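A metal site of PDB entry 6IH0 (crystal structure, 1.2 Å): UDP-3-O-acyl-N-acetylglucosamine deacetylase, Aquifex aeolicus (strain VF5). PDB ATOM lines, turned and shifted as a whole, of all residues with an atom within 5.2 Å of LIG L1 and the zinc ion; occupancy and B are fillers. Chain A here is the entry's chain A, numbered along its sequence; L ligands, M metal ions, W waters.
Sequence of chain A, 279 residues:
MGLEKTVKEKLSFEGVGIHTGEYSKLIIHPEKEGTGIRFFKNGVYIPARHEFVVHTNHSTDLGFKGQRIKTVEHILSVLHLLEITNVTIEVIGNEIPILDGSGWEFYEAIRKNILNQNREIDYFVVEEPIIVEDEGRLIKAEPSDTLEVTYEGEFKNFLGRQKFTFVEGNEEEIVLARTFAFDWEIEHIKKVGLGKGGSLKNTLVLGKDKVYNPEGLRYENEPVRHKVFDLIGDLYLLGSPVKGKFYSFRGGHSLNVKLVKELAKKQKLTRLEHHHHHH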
ATOM      1  N   ILE A  18      11.135 -18.847 -20.120  1.00  0.00           N
ATOM      2  CA  ILE A  18      12.424 -18.863 -19.430  1.00  0.00           C
ATOM      3  C   ILE A  18      13.599 -18.934 -20.399  1.00  0.00           C
ATOM      4  O   ILE A  18      14.667 -18.354 -20.148  1.00  0.00           O
ATOM      5  CB  ILE A  18      12.474 -19.976 -18.362  1.00  0.00           C
ATOM      6  CG1 ILE A  18      13.674 -19.771 -17.437  1.00  0.00           C
ATOM      7  CG2 ILE A  18      12.589 -21.341 -18.986  1.00  0.00           C
ATOM      8  CD1 ILE A  18      13.413 -18.837 -16.324  1.00  0.00           C
ATOM      9  N   HIS A  19      13.462 -19.673 -21.502  1.00  0.00           N
ATOM     10  CA  HIS A  19      14.566 -19.877 -22.423  1.00  0.00           C
ATOM     11  C   HIS A  19      14.594 -18.894 -23.578  1.00  0.00           C
ATOM     12  O   HIS A  19      15.672 -18.394 -23.930  1.00  0.00           O
ATOM     13  CB  HIS A  19      14.615 -21.311 -22.936  1.00  0.00           C
ATOM     14  CG  HIS A  19      15.000 -22.265 -21.864  1.00  0.00           C
ATOM     15  ND1 HIS A  19      16.133 -22.082 -21.104  1.00  0.00           N
ATOM     16  CD2 HIS A  19      14.377 -23.359 -21.367  1.00  0.00           C
ATOM     17  CE1 HIS A  19      16.209 -23.044 -20.205  1.00  0.00           C
ATOM     18  NE2 HIS A  19      15.154 -23.834 -20.343  1.00  0.00           N
ATOM     19  N   HIS A  58      17.849 -28.841 -20.961  1.00  0.00           N
ATOM     20  CA  HIS A  58      17.375 -27.739 -20.120  1.00  0.00           C
ATOM     21  C   HIS A  58      15.873 -27.519 -20.192  1.00  0.00           C
ATOM     22  O   HIS A  58      15.342 -26.732 -19.397  1.00  0.00           O
ATOM     23  CB  HIS A  58      18.113 -26.407 -20.335  1.00  0.00           C
ATOM     24  CG  HIS A  58      19.586 -26.504 -20.091  1.00  0.00           C
ATOM     25  ND1 HIS A  58      20.141 -26.445 -18.834  1.00  0.00           N
ATOM     26  CD2 HIS A  58      20.609 -26.718 -20.950  1.00  0.00           C
ATOM     27  CE1 HIS A  58      21.454 -26.580 -18.937  1.00  0.00           C
ATOM     28  NE2 HIS A  58      21.764 -26.745 -20.208  1.00  0.00           N
ATOM     29  N   SER A  59      15.168 -28.162 -21.105  1.00  0.00           N
ATOM     30  CA  SER A  59      13.710 -28.161 -21.136  1.00  0.00           C
ATOM     31  C   SER A  59      13.302 -29.332 -22.024  1.00  0.00           C
ATOM     32  O   SER A  59      14.128 -29.922 -22.716  1.00  0.00           O
ATOM     33  CB  SER A  59      13.166 -26.849 -21.696  1.00  0.00           C
ATOM     34  OG  SER A  59      13.597 -26.644 -23.048  1.00  0.00           O
ATOM     35  N   GLU A  73       7.212 -29.004 -19.856  1.00  0.00           N
ATOM     36  CA  GLU A  73       7.217 -29.928 -18.726  1.00  0.00           C
ATOM     37  C   GLU A  73       6.400 -29.433 -17.532  1.00  0.00           C
ATOM     38  O   GLU A  73       5.819 -30.240 -16.807  1.00  0.00           O
ATOM     39  CB  GLU A  73       8.639 -30.263 -18.316  1.00  0.00           C
ATOM     40  CG  GLU A  73       9.493 -29.052 -17.904  1.00  0.00           C
ATOM     41  CD  GLU A  73      10.325 -28.461 -19.039  1.00  0.00           C
ATOM     42  OE1 GLU A  73       9.964 -28.629 -20.232  1.00  0.00           O
ATOM     43  OE2 GLU A  73      11.346 -27.801 -18.751  1.00  0.00           O
ATOM     44  N   HIS A  74       6.358 -28.117 -17.287  1.00  0.00           N
ATOM     45  CA  HIS A  74       5.702 -27.629 -16.076  1.00  0.00           C
ATOM     46  C   HIS A  74       4.186 -27.650 -16.231  1.00  0.00           C
ATOM     47  O   HIS A  74       3.477 -28.118 -15.321  1.00  0.00           O
ATOM     48  CB  HIS A  74       6.215 -26.246 -15.687  1.00  0.00           C
ATOM     49  CG  HIS A  74       7.706 -26.190 -15.547  1.00  0.00           C
ATOM     50  ND1 HIS A  74       8.469 -25.191 -16.109  1.00  0.00           N
ATOM     51  CD2 HIS A  74       8.591 -27.051 -14.984  1.00  0.00           C
ATOM     52  CE1 HIS A  74       9.752 -25.410 -15.850  1.00  0.00           C
ATOM     53  NE2 HIS A  74       9.843 -26.519 -15.141  1.00  0.00           N
ATOM     54  N   THR A 179      12.008 -23.748 -10.610  1.00  0.00           N
ATOM     55  CA  THR A 179      13.199 -24.045 -11.361  1.00  0.00           C
ATOM     56  C   THR A 179      14.399 -23.314 -10.742  1.00  0.00           C
ATOM     57  O   THR A 179      14.248 -22.336 -10.009  1.00  0.00           O
ATOM     58  CB  THR A 179      13.004 -23.667 -12.825  1.00  0.00           C
ATOM     59  OG1 THR A 179      14.036 -24.273 -13.612  1.00  0.00           O
ATOM     60  CG2 THR A 179      13.008 -22.168 -13.040  1.00  0.00           C
ATOM     61  N   PHE A 180      15.592 -23.801 -11.054  1.00  0.00           N
ATOM     62  CA  PHE A 180      16.790 -23.340 -10.388  1.00  0.00           C
ATOM     63  C   PHE A 180      17.961 -23.389 -11.351  1.00  0.00           C
ATOM     64  O   PHE A 180      17.922 -24.074 -12.382  1.00  0.00           O
ATOM     65  CB  PHE A 180      17.074 -24.150  -9.109  1.00  0.00           C
ATOM     66  CG  PHE A 180      17.283 -25.617  -9.359  1.00  0.00           C
ATOM     67  CD1 PHE A 180      16.207 -26.484  -9.431  1.00  0.00           C
ATOM     68  CD2 PHE A 180      18.564 -26.126  -9.523  1.00  0.00           C
ATOM     69  CE1 PHE A 180      16.405 -27.844  -9.653  1.00  0.00           C
ATOM     70  CE2 PHE A 180      18.758 -27.482  -9.762  1.00  0.00           C
ATOM     71  CZ  PHE A 180      17.669 -28.340  -9.815  1.00  0.00           C
ATOM     72  N   ALA A 181      19.014 -22.651 -10.998  1.00  0.00           N
ATOM     73  CA  ALA A 181      20.222 -22.584 -11.797  1.00  0.00           C
ATOM     74  C   ALA A 181      21.385 -22.234 -10.890  1.00  0.00           C
ATOM     75  O   ALA A 181      21.220 -21.614  -9.839  1.00  0.00           O
ATOM     76  CB  ALA A 181      20.113 -21.548 -12.916  1.00  0.00           C
ATOM     77  N   ILE A 186      25.517 -20.481 -15.594  1.00  0.00           N
ATOM     78  CA  ILE A 186      24.583 -19.638 -16.338  1.00  0.00           C
ATOM     79  C   ILE A 186      25.227 -19.091 -17.605  1.00  0.00           C
ATOM     80  O   ILE A 186      24.568 -18.981 -18.648  1.00  0.00           O
ATOM     81  CB  ILE A 186      23.973 -18.565 -15.431  1.00  0.00           C
ATOM     82  CG1 ILE A 186      22.948 -19.196 -14.481  1.00  0.00           C
ATOM     83  CG2 ILE A 186      23.322 -17.457 -16.262  1.00  0.00           C
ATOM     84  CD1 ILE A 186      22.485 -18.287 -13.370  1.00  0.00           C
ATOM     85  N   ILE A 189      24.906 -21.670 -20.276  1.00  0.00           N
ATOM     86  CA  ILE A 189      23.509 -21.828 -20.685  1.00  0.00           C
ATOM     87  C   ILE A 189      23.105 -20.710 -21.634  1.00  0.00           C
ATOM     88  O   ILE A 189      22.460 -20.948 -22.670  1.00  0.00           O
ATOM     89  CB  ILE A 189      22.598 -21.919 -19.449  1.00  0.00           C
ATOM     90  CG1 ILE A 189      22.891 -23.194 -18.667  1.00  0.00           C
ATOM     91  CG2 ILE A 189      21.142 -21.859 -19.859  1.00  0.00           C
ATOM     92  CD1 ILE A 189      22.307 -23.230 -17.261  1.00  0.00           C
ATOM     93  N   LYS A 190      23.495 -19.469 -21.318  1.00  0.00           N
ATOM     94  CA  LYS A 190      23.189 -18.377 -22.219  1.00  0.00           C
ATOM     95  C   LYS A 190      23.947 -18.501 -23.532  1.00  0.00           C
ATOM     96  O   LYS A 190      23.399 -18.230 -24.610  1.00  0.00           O
ATOM     97  CB  LYS A 190      23.458 -17.038 -21.525  1.00  0.00           C
ATOM     98  CG  LYS A 190      22.484 -16.775 -20.381  1.00  0.00           C
ATOM     99  CD  LYS A 190      22.679 -15.407 -19.764  1.00  0.00           C
ATOM    100  CE  LYS A 190      21.642 -15.144 -18.670  1.00  0.00           C
ATOM    101  NZ  LYS A 190      20.297 -14.807 -19.240  1.00  0.00           N
ATOM    102  N   GLY A 195      18.034 -19.831 -21.516  1.00  0.00           N
ATOM    103  CA  GLY A 195      17.972 -19.004 -20.315  1.00  0.00           C
ATOM    104  C   GLY A 195      17.739 -17.533 -20.529  1.00  0.00           C
ATOM    105  O   GLY A 195      17.968 -16.742 -19.603  1.00  0.00           O
ATOM    106  N   GLY A 198      15.514 -15.918 -17.875  1.00  0.00           N
ATOM    107  CA  GLY A 198      15.774 -16.220 -16.478  1.00  0.00           C
ATOM    108  C   GLY A 198      16.099 -14.985 -15.670  1.00  0.00           C
ATOM    109  O   GLY A 198      16.833 -14.105 -16.117  1.00  0.00           O
ATOM    110  N   SER A 199      15.567 -14.938 -14.453  1.00  0.00           N
ATOM    111  CA  SER A 199      15.835 -13.824 -13.554  1.00  0.00           C
ATOM    112  C   SER A 199      15.531 -14.303 -12.141  1.00  0.00           C
ATOM    113  O   SER A 199      14.995 -15.396 -11.936  1.00  0.00           O
ATOM    114  CB  SER A 199      14.952 -12.619 -13.872  1.00  0.00           C
ATOM    115  OG  SER A 199      13.638 -12.853 -13.402  1.00  0.00           O
ATOM    116  N   LEU A 200      15.846 -13.459 -11.170  1.00  0.00           N
ATOM    117  CA  LEU A 200      15.510 -13.793  -9.788  1.00  0.00           C
ATOM    118  C   LEU A 200      14.016 -13.764  -9.540  1.00  0.00           C
ATOM    119  O   LEU A 200      13.585 -14.189  -8.460  1.00  0.00           O
ATOM    120  CB  LEU A 200      16.239 -12.861  -8.833  1.00  0.00           C
ATOM    121  CG  LEU A 200      17.772 -12.915  -8.889  1.00  0.00           C
ATOM    122  CD1 LEU A 200      18.354 -11.938  -7.878  1.00  0.00           C
ATOM    123  CD2 LEU A 200      18.267 -14.320  -8.631  1.00  0.00           C
ATOM    124  N   THR A 203      13.482 -17.798 -11.111  1.00  0.00           N
ATOM    125  CA  THR A 203      14.472 -18.858 -10.971  1.00  0.00           C
ATOM    126  C   THR A 203      15.132 -18.707  -9.610  1.00  0.00           C
ATOM    127  O   THR A 203      15.477 -17.601  -9.192  1.00  0.00           O
ATOM    128  CB  THR A 203      15.553 -18.721 -12.051  1.00  0.00           C
ATOM    129  OG1 THR A 203      14.941 -18.754 -13.341  1.00  0.00           O
ATOM    130  CG2 THR A 203      16.574 -19.831 -11.961  1.00  0.00           C
ATOM    131  N   VAL A 205      18.384 -18.955  -7.937  1.00  0.00           N
ATOM    132  CA  VAL A 205      19.757 -18.885  -8.412  1.00  0.00           C
ATOM    133  C   VAL A 205      20.695 -19.091  -7.238  1.00  0.00           C
ATOM    134  O   VAL A 205      20.641 -18.342  -6.260  1.00  0.00           O
ATOM    135  CB  VAL A 205      20.045 -17.574  -9.168  1.00  0.00           C
ATOM    136  CG1 VAL A 205      21.493 -17.550  -9.618  1.00  0.00           C
ATOM    137  CG2 VAL A 205      19.114 -17.452 -10.362  1.00  0.00           C
ATOM    138  N   TYR A 212      21.136 -16.305  -4.232  1.00  0.00           N
ATOM    139  CA  TYR A 212      21.022 -14.959  -4.788  1.00  0.00           C
ATOM    140  C   TYR A 212      19.666 -14.328  -4.491  1.00  0.00           C
ATOM    141  O   TYR A 212      19.577 -13.113  -4.264  1.00  0.00           O
ATOM    142  CB  TYR A 212      21.287 -14.977  -6.288  1.00  0.00           C
ATOM    143  CG  TYR A 212      22.731 -15.105  -6.675  1.00  0.00           C
ATOM    144  CD1 TYR A 212      23.400 -16.311  -6.564  1.00  0.00           C
ATOM    145  CD2 TYR A 212      23.443 -14.013  -7.171  1.00  0.00           C
ATOM    146  CE1 TYR A 212      24.732 -16.440  -6.921  1.00  0.00           C
ATOM    147  CE2 TYR A 212      24.775 -14.125  -7.543  1.00  0.00           C
ATOM    148  CZ  TYR A 212      25.413 -15.337  -7.413  1.00  0.00           C
ATOM    149  OH  TYR A 212      26.736 -15.456  -7.765  1.00  0.00           O
ATOM    150  N   HIS A 226      11.583 -29.688  -7.268  1.00  0.00           N
ATOM    151  CA  HIS A 226      11.357 -29.258  -8.644  1.00  0.00           C
ATOM    152  C   HIS A 226      11.703 -30.354  -9.634  1.00  0.00           C
ATOM    153  O   HIS A 226      11.005 -30.531 -10.642  1.00  0.00           O
ATOM    154  CB  HIS A 226      12.131 -27.984  -8.968  1.00  0.00           C
ATOM    155  CG  HIS A 226      11.773 -27.465 -10.313  1.00  0.00           C
ATOM    156  ND1 HIS A 226      10.628 -26.733 -10.526  1.00  0.00           N
ATOM    157  CD2 HIS A 226      12.310 -27.696 -11.531  1.00  0.00           C
ATOM    158  CE1 HIS A 226      10.505 -26.487 -11.825  1.00  0.00           C
ATOM    159  NE2 HIS A 226      11.505 -27.066 -12.451  1.00  0.00           N
ATOM    160  N   LYS A 227      12.781 -31.095  -9.400  1.00  0.00           N
ATOM    161  CA  LYS A 227      13.149 -32.179 -10.307  1.00  0.00           C
ATOM    162  C   LYS A 227      12.094 -33.282 -10.322  1.00  0.00           C
ATOM    163  O   LYS A 227      11.857 -33.893 -11.375  1.00  0.00           O
ATOM    164  CB  LYS A 227      14.530 -32.726  -9.967  1.00  0.00           C
ATOM    165  CG  LYS A 227      15.650 -31.717 -10.162  1.00  0.00           C
ATOM    166  CD  LYS A 227      15.923 -31.446 -11.633  1.00  0.00           C
ATOM    167  CE  LYS A 227      16.609 -32.627 -12.292  1.00  0.00           C
ATOM    168  NZ  LYS A 227      17.213 -32.307 -13.614  1.00  0.00           N
ATOM    169  N   ASP A 230       9.377 -31.875 -12.521  1.00  0.00           N
ATOM    170  CA  ASP A 230       9.764 -32.018 -13.930  1.00  0.00           C
ATOM    171  C   ASP A 230       9.510 -33.435 -14.426  1.00  0.00           C
ATOM    172  O   ASP A 230       9.009 -33.637 -15.547  1.00  0.00           O
ATOM    173  CB  ASP A 230      11.261 -31.732 -14.105  1.00  0.00           C
ATOM    174  CG  ASP A 230      11.613 -30.255 -14.135  1.00  0.00           C
ATOM    175  OD1 ASP A 230      10.749 -29.377 -14.333  1.00  0.00           O
ATOM    176  OD2 ASP A 230      12.831 -29.990 -13.973  1.00  0.00           O
ATOM    177  N   HIS A 253      15.840 -34.141 -18.221  1.00  0.00           N
ATOM    178  CA  HIS A 253      14.828 -34.367 -19.261  1.00  0.00           C
ATOM    179  C   HIS A 253      15.255 -35.438 -20.260  1.00  0.00           C
ATOM    180  O   HIS A 253      14.411 -36.215 -20.715  1.00  0.00           O
ATOM    181  CB  HIS A 253      14.503 -33.091 -20.016  1.00  0.00           C
ATOM    182  CG  HIS A 253      14.010 -31.996 -19.129  1.00  0.00           C
ATOM    183  ND1 HIS A 253      12.859 -32.101 -18.378  1.00  0.00           N
ATOM    184  CD2 HIS A 253      14.534 -30.774 -18.866  1.00  0.00           C
ATOM    185  CE1 HIS A 253      12.704 -30.979 -17.690  1.00  0.00           C
ATOM    186  NE2 HIS A 253      13.703 -30.165 -17.966  1.00  0.00           N
HETATM  187  C1  LIG L   1      21.411 -14.172 -13.895  1.00  0.00           C
HETATM  188  C2  LIG L   1      20.665 -14.474 -12.599  1.00  0.00           C
HETATM  189  C3  LIG L   1      19.890 -14.370 -13.913  1.00  0.00           C
HETATM  190  C4  LIG L   1      20.464 -13.291 -11.634  1.00  0.00           C
HETATM  191  C5  LIG L   1      19.423 -15.717 -14.465  1.00  0.00           C
HETATM  192  C6  LIG L   1      16.416 -27.704 -14.613  1.00  0.00           C
HETATM  193  C7  LIG L   1      15.643 -26.897 -15.683  1.00  0.00           C
HETATM  194  C8  LIG L   1      19.051 -16.763 -14.868  1.00  0.00           C
HETATM  195  C9  LIG L   1      15.841 -29.136 -14.538  1.00  0.00           C
HETATM  196  C10 LIG L   1      16.309 -27.046 -13.213  1.00  0.00           C
HETATM  197  C11 LIG L   1      14.157 -27.100 -15.540  1.00  0.00           C
HETATM  198  C12 LIG L   1      16.900 -24.937 -16.482  1.00  0.00           C
HETATM  199  C13 LIG L   1      18.583 -18.129 -15.339  1.00  0.00           C
HETATM  200  C14 LIG L   1      17.161 -23.484 -16.267  1.00  0.00           C
HETATM  201  C15 LIG L   1      18.495 -22.999 -16.794  1.00  0.00           C
HETATM  202  C16 LIG L   1      16.198 -22.616 -15.468  1.00  0.00           C
HETATM  203  C17 LIG L   1      17.895 -20.684 -15.790  1.00  0.00           C
HETATM  204  C18 LIG L   1      18.281 -19.241 -15.555  1.00  0.00           C
HETATM  205  C19 LIG L   1      18.867 -21.559 -16.556  1.00  0.00           C
HETATM  206  C20 LIG L   1      16.571 -21.176 -15.230  1.00  0.00           C
HETATM  207  N1  LIG L   1      15.930 -25.505 -15.588  1.00  0.00           N
HETATM  208  N2  LIG L   1      17.848 -27.749 -14.964  1.00  0.00           N
HETATM  209  N3  LIG L   1      13.591 -27.799 -16.631  1.00  0.00           N
HETATM  210  O1  LIG L   1      21.600 -13.156 -10.807  1.00  0.00           O
HETATM  211  O2  LIG L   1      13.460 -26.714 -14.636  1.00  0.00           O
HETATM  212  O3  LIG L   1      17.550 -25.609 -17.221  1.00  0.00           O
HETATM  213  O4  LIG L   1      12.217 -27.997 -16.480  1.00  0.00           O
HETATM  214  C1  LG2 L   2      22.330 -31.987 -17.767  1.00  0.00           C
HETATM  215  C2  LG2 L   2      17.899 -30.880 -17.630  1.00  0.00           C
HETATM  216  C3  LG2 L   2      24.614 -29.974 -17.955  1.00  0.00           C
HETATM  217  C4  LG2 L   2      19.966 -30.893 -16.691  1.00  0.00           C
HETATM  218  C5  LG2 L   2      16.907 -31.660 -16.791  1.00  0.00           C
HETATM  219  C6  LG2 L   2      17.754 -29.385 -17.366  1.00  0.00           C
HETATM  220  C7  LG2 L   2      17.743 -31.153 -19.091  1.00  0.00           C
HETATM  221  C8  LG2 L   2      26.110 -29.915 -16.096  1.00  0.00           C
HETATM  222  C9  LG2 L   2      22.264 -30.496 -17.408  1.00  0.00           C
HETATM  223  C10 LG2 L   2      23.173 -29.672 -18.349  1.00  0.00           C
HETATM  224  C11 LG2 L   2      22.710 -30.279 -15.969  1.00  0.00           C
HETATM  225  N1  LG2 L   2      20.892 -30.053 -17.462  1.00  0.00           N
HETATM  226  N2  LG2 L   2      22.965 -30.052 -19.717  1.00  0.00           N
HETATM  227  O1  LG2 L   2      19.080 -31.599 -17.443  1.00  0.00           O
HETATM  228  O2  LG2 L   2      25.308 -29.182 -16.999  1.00  0.00           O
HETATM  229  O3  LG2 L   2      25.163 -30.892 -18.455  1.00  0.00           O
HETATM  230  O4  LG2 L   2      19.935 -31.023 -15.502  1.00  0.00           O
HETATM  231 ZN    ZN M   1      11.553 -27.514 -14.502  1.00  0.00          ZN
HETATM  232  O   HOH W   1      19.347 -29.929 -13.310  1.00  0.00           O
HETATM  233  O   HOH W   2      13.060 -25.431 -18.552  1.00  0.00           O
HETATM  234  O   HOH W   3      19.467 -25.326 -14.178  1.00  0.00           O
HETATM  235  O   HOH W   4      14.480 -32.139 -14.873  1.00  0.00           O
HETATM  236  O   HOH W   5      12.531 -23.900 -16.274  1.00  0.00           O
HETATM  237  O   HOH W   6      20.361 -26.510 -16.245  1.00  0.00           O
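Water W3 lies within hydrogen-bond range of O of Phe 180 (2.7 Å) and N2 of LIG L1 (3.0 Å).
Water W6 lies within hydrogen-bond range of a ring nitrogen (ND1) of His 58 (2.6 Å) and a nitrogen (N2) of LIG L1 (3.1 Å).
Water W2 lies within hydrogen-bond range of O of His 58, OE2 of Glu 73, N3 of LIG L1 and NE2 of His 19.
Water W1 lies within hydrogen-bond range of an oxygen (O4) of LG2 L2 (2.5 Å), a nitrogen (N2) of LIG L1 (3.1 Å) and the side-chain amino group (NZ) of Lys 227 (3.2 Å).
Water W4 bridges the side-chain carboxylate of Asp 230 (2.9 Å) and the side-chain amino group of Lys 227 (3.0 Å).
Of the 23 residues printed, 3 come within 4 Å of the zinc ion.
A ring nitrogen (ND1) of His 58 sits at hydrogen-bond distance from an oxygen (O3) of LIG L1 (3.2 Å).
A ring nitrogen (NE2) of His 253 sits at hydrogen-bond distance from a nitrogen (N3) of LIG L1, 2.7 Å away.
The side-chain carboxylate (OE2) of Glu 73 is in hydrogen-bond range of a nitrogen (N3) of LIG L1, 3.1 Å away.
The backbone carbonyl oxygen (O) of His 58 sits at hydrogen-bond distance from a nitrogen (N3) of LIG L1 (3.4 Å).
The side-chain hydroxyl (OG1) of Thr 179 sits at hydrogen-bond distance from a nitrogen (N1) of LIG L1, at 3.0 Å.
CG1 of Ile 18 touches C20 of LIG L1, 3.9 Å away.
Phe 180 touches LIG L1.
CB of Ala 181 touches C17 of LIG L1 (3.7 Å).
Ile 189 touches LIG L1.
O of Gly 198 touches C5 of LIG L1 (3.5 Å).
Ser 199 touches LIG L1.
Leu 200 touches LIG L1.
Thr 203 touches LIG L1.
Lys 227 touches LIG L1 (NZ to C9, 3.6 Å).
Hydrophobic or aromatic side chains within 4 Å of LIG L1: Ile 18, His 58, His 74, Phe 180, Ala 181, Ile 189, Leu 200, His 226 and His 253.
16 residues have an atom within 4 Å of LIG L1: Ile 18, His 58, Glu 73, His 74, Thr 179, Phe 180, Ala 181, Ile 189, Gly 198, Ser 199, Leu 200, Thr 203, His 226, Lys 227, Asp 230 and His 253.
Along chain A the residues within 4 Å of LIG L1 span positions 18 to 253.
The nearest printed residue that does not touch LIG L1 is Val 205 (4.03 Å).
NE2 of His 19 sits at hydrogen-bond distance from O of His 58.
The backbone carbonyl oxygen (O) of Ile 18 is in hydrogen-bond range of the backbone NH (N) of Gly 198, 3.4 Å away.
OE2 of Glu 73 is in hydrogen-bond range of NE2 of His 253, at 3.4 Å.
The backbone NH (N) of Thr 179 sits at hydrogen-bond distance from a ring nitrogen (ND1) of His 226 (3.3 Å).
The zinc ion is bound by OD1 of Asp 230 (2.0 Å), O2 of LIG L1 (2.1 Å), NE2 of His 74 (2.1 Å), NE2 of His 226 (2.1 Å) and O4 of LIG L1 (2.1 Å).
Slightly farther from the zinc ion lies OD2 of Asp 230 (2.8 Å).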
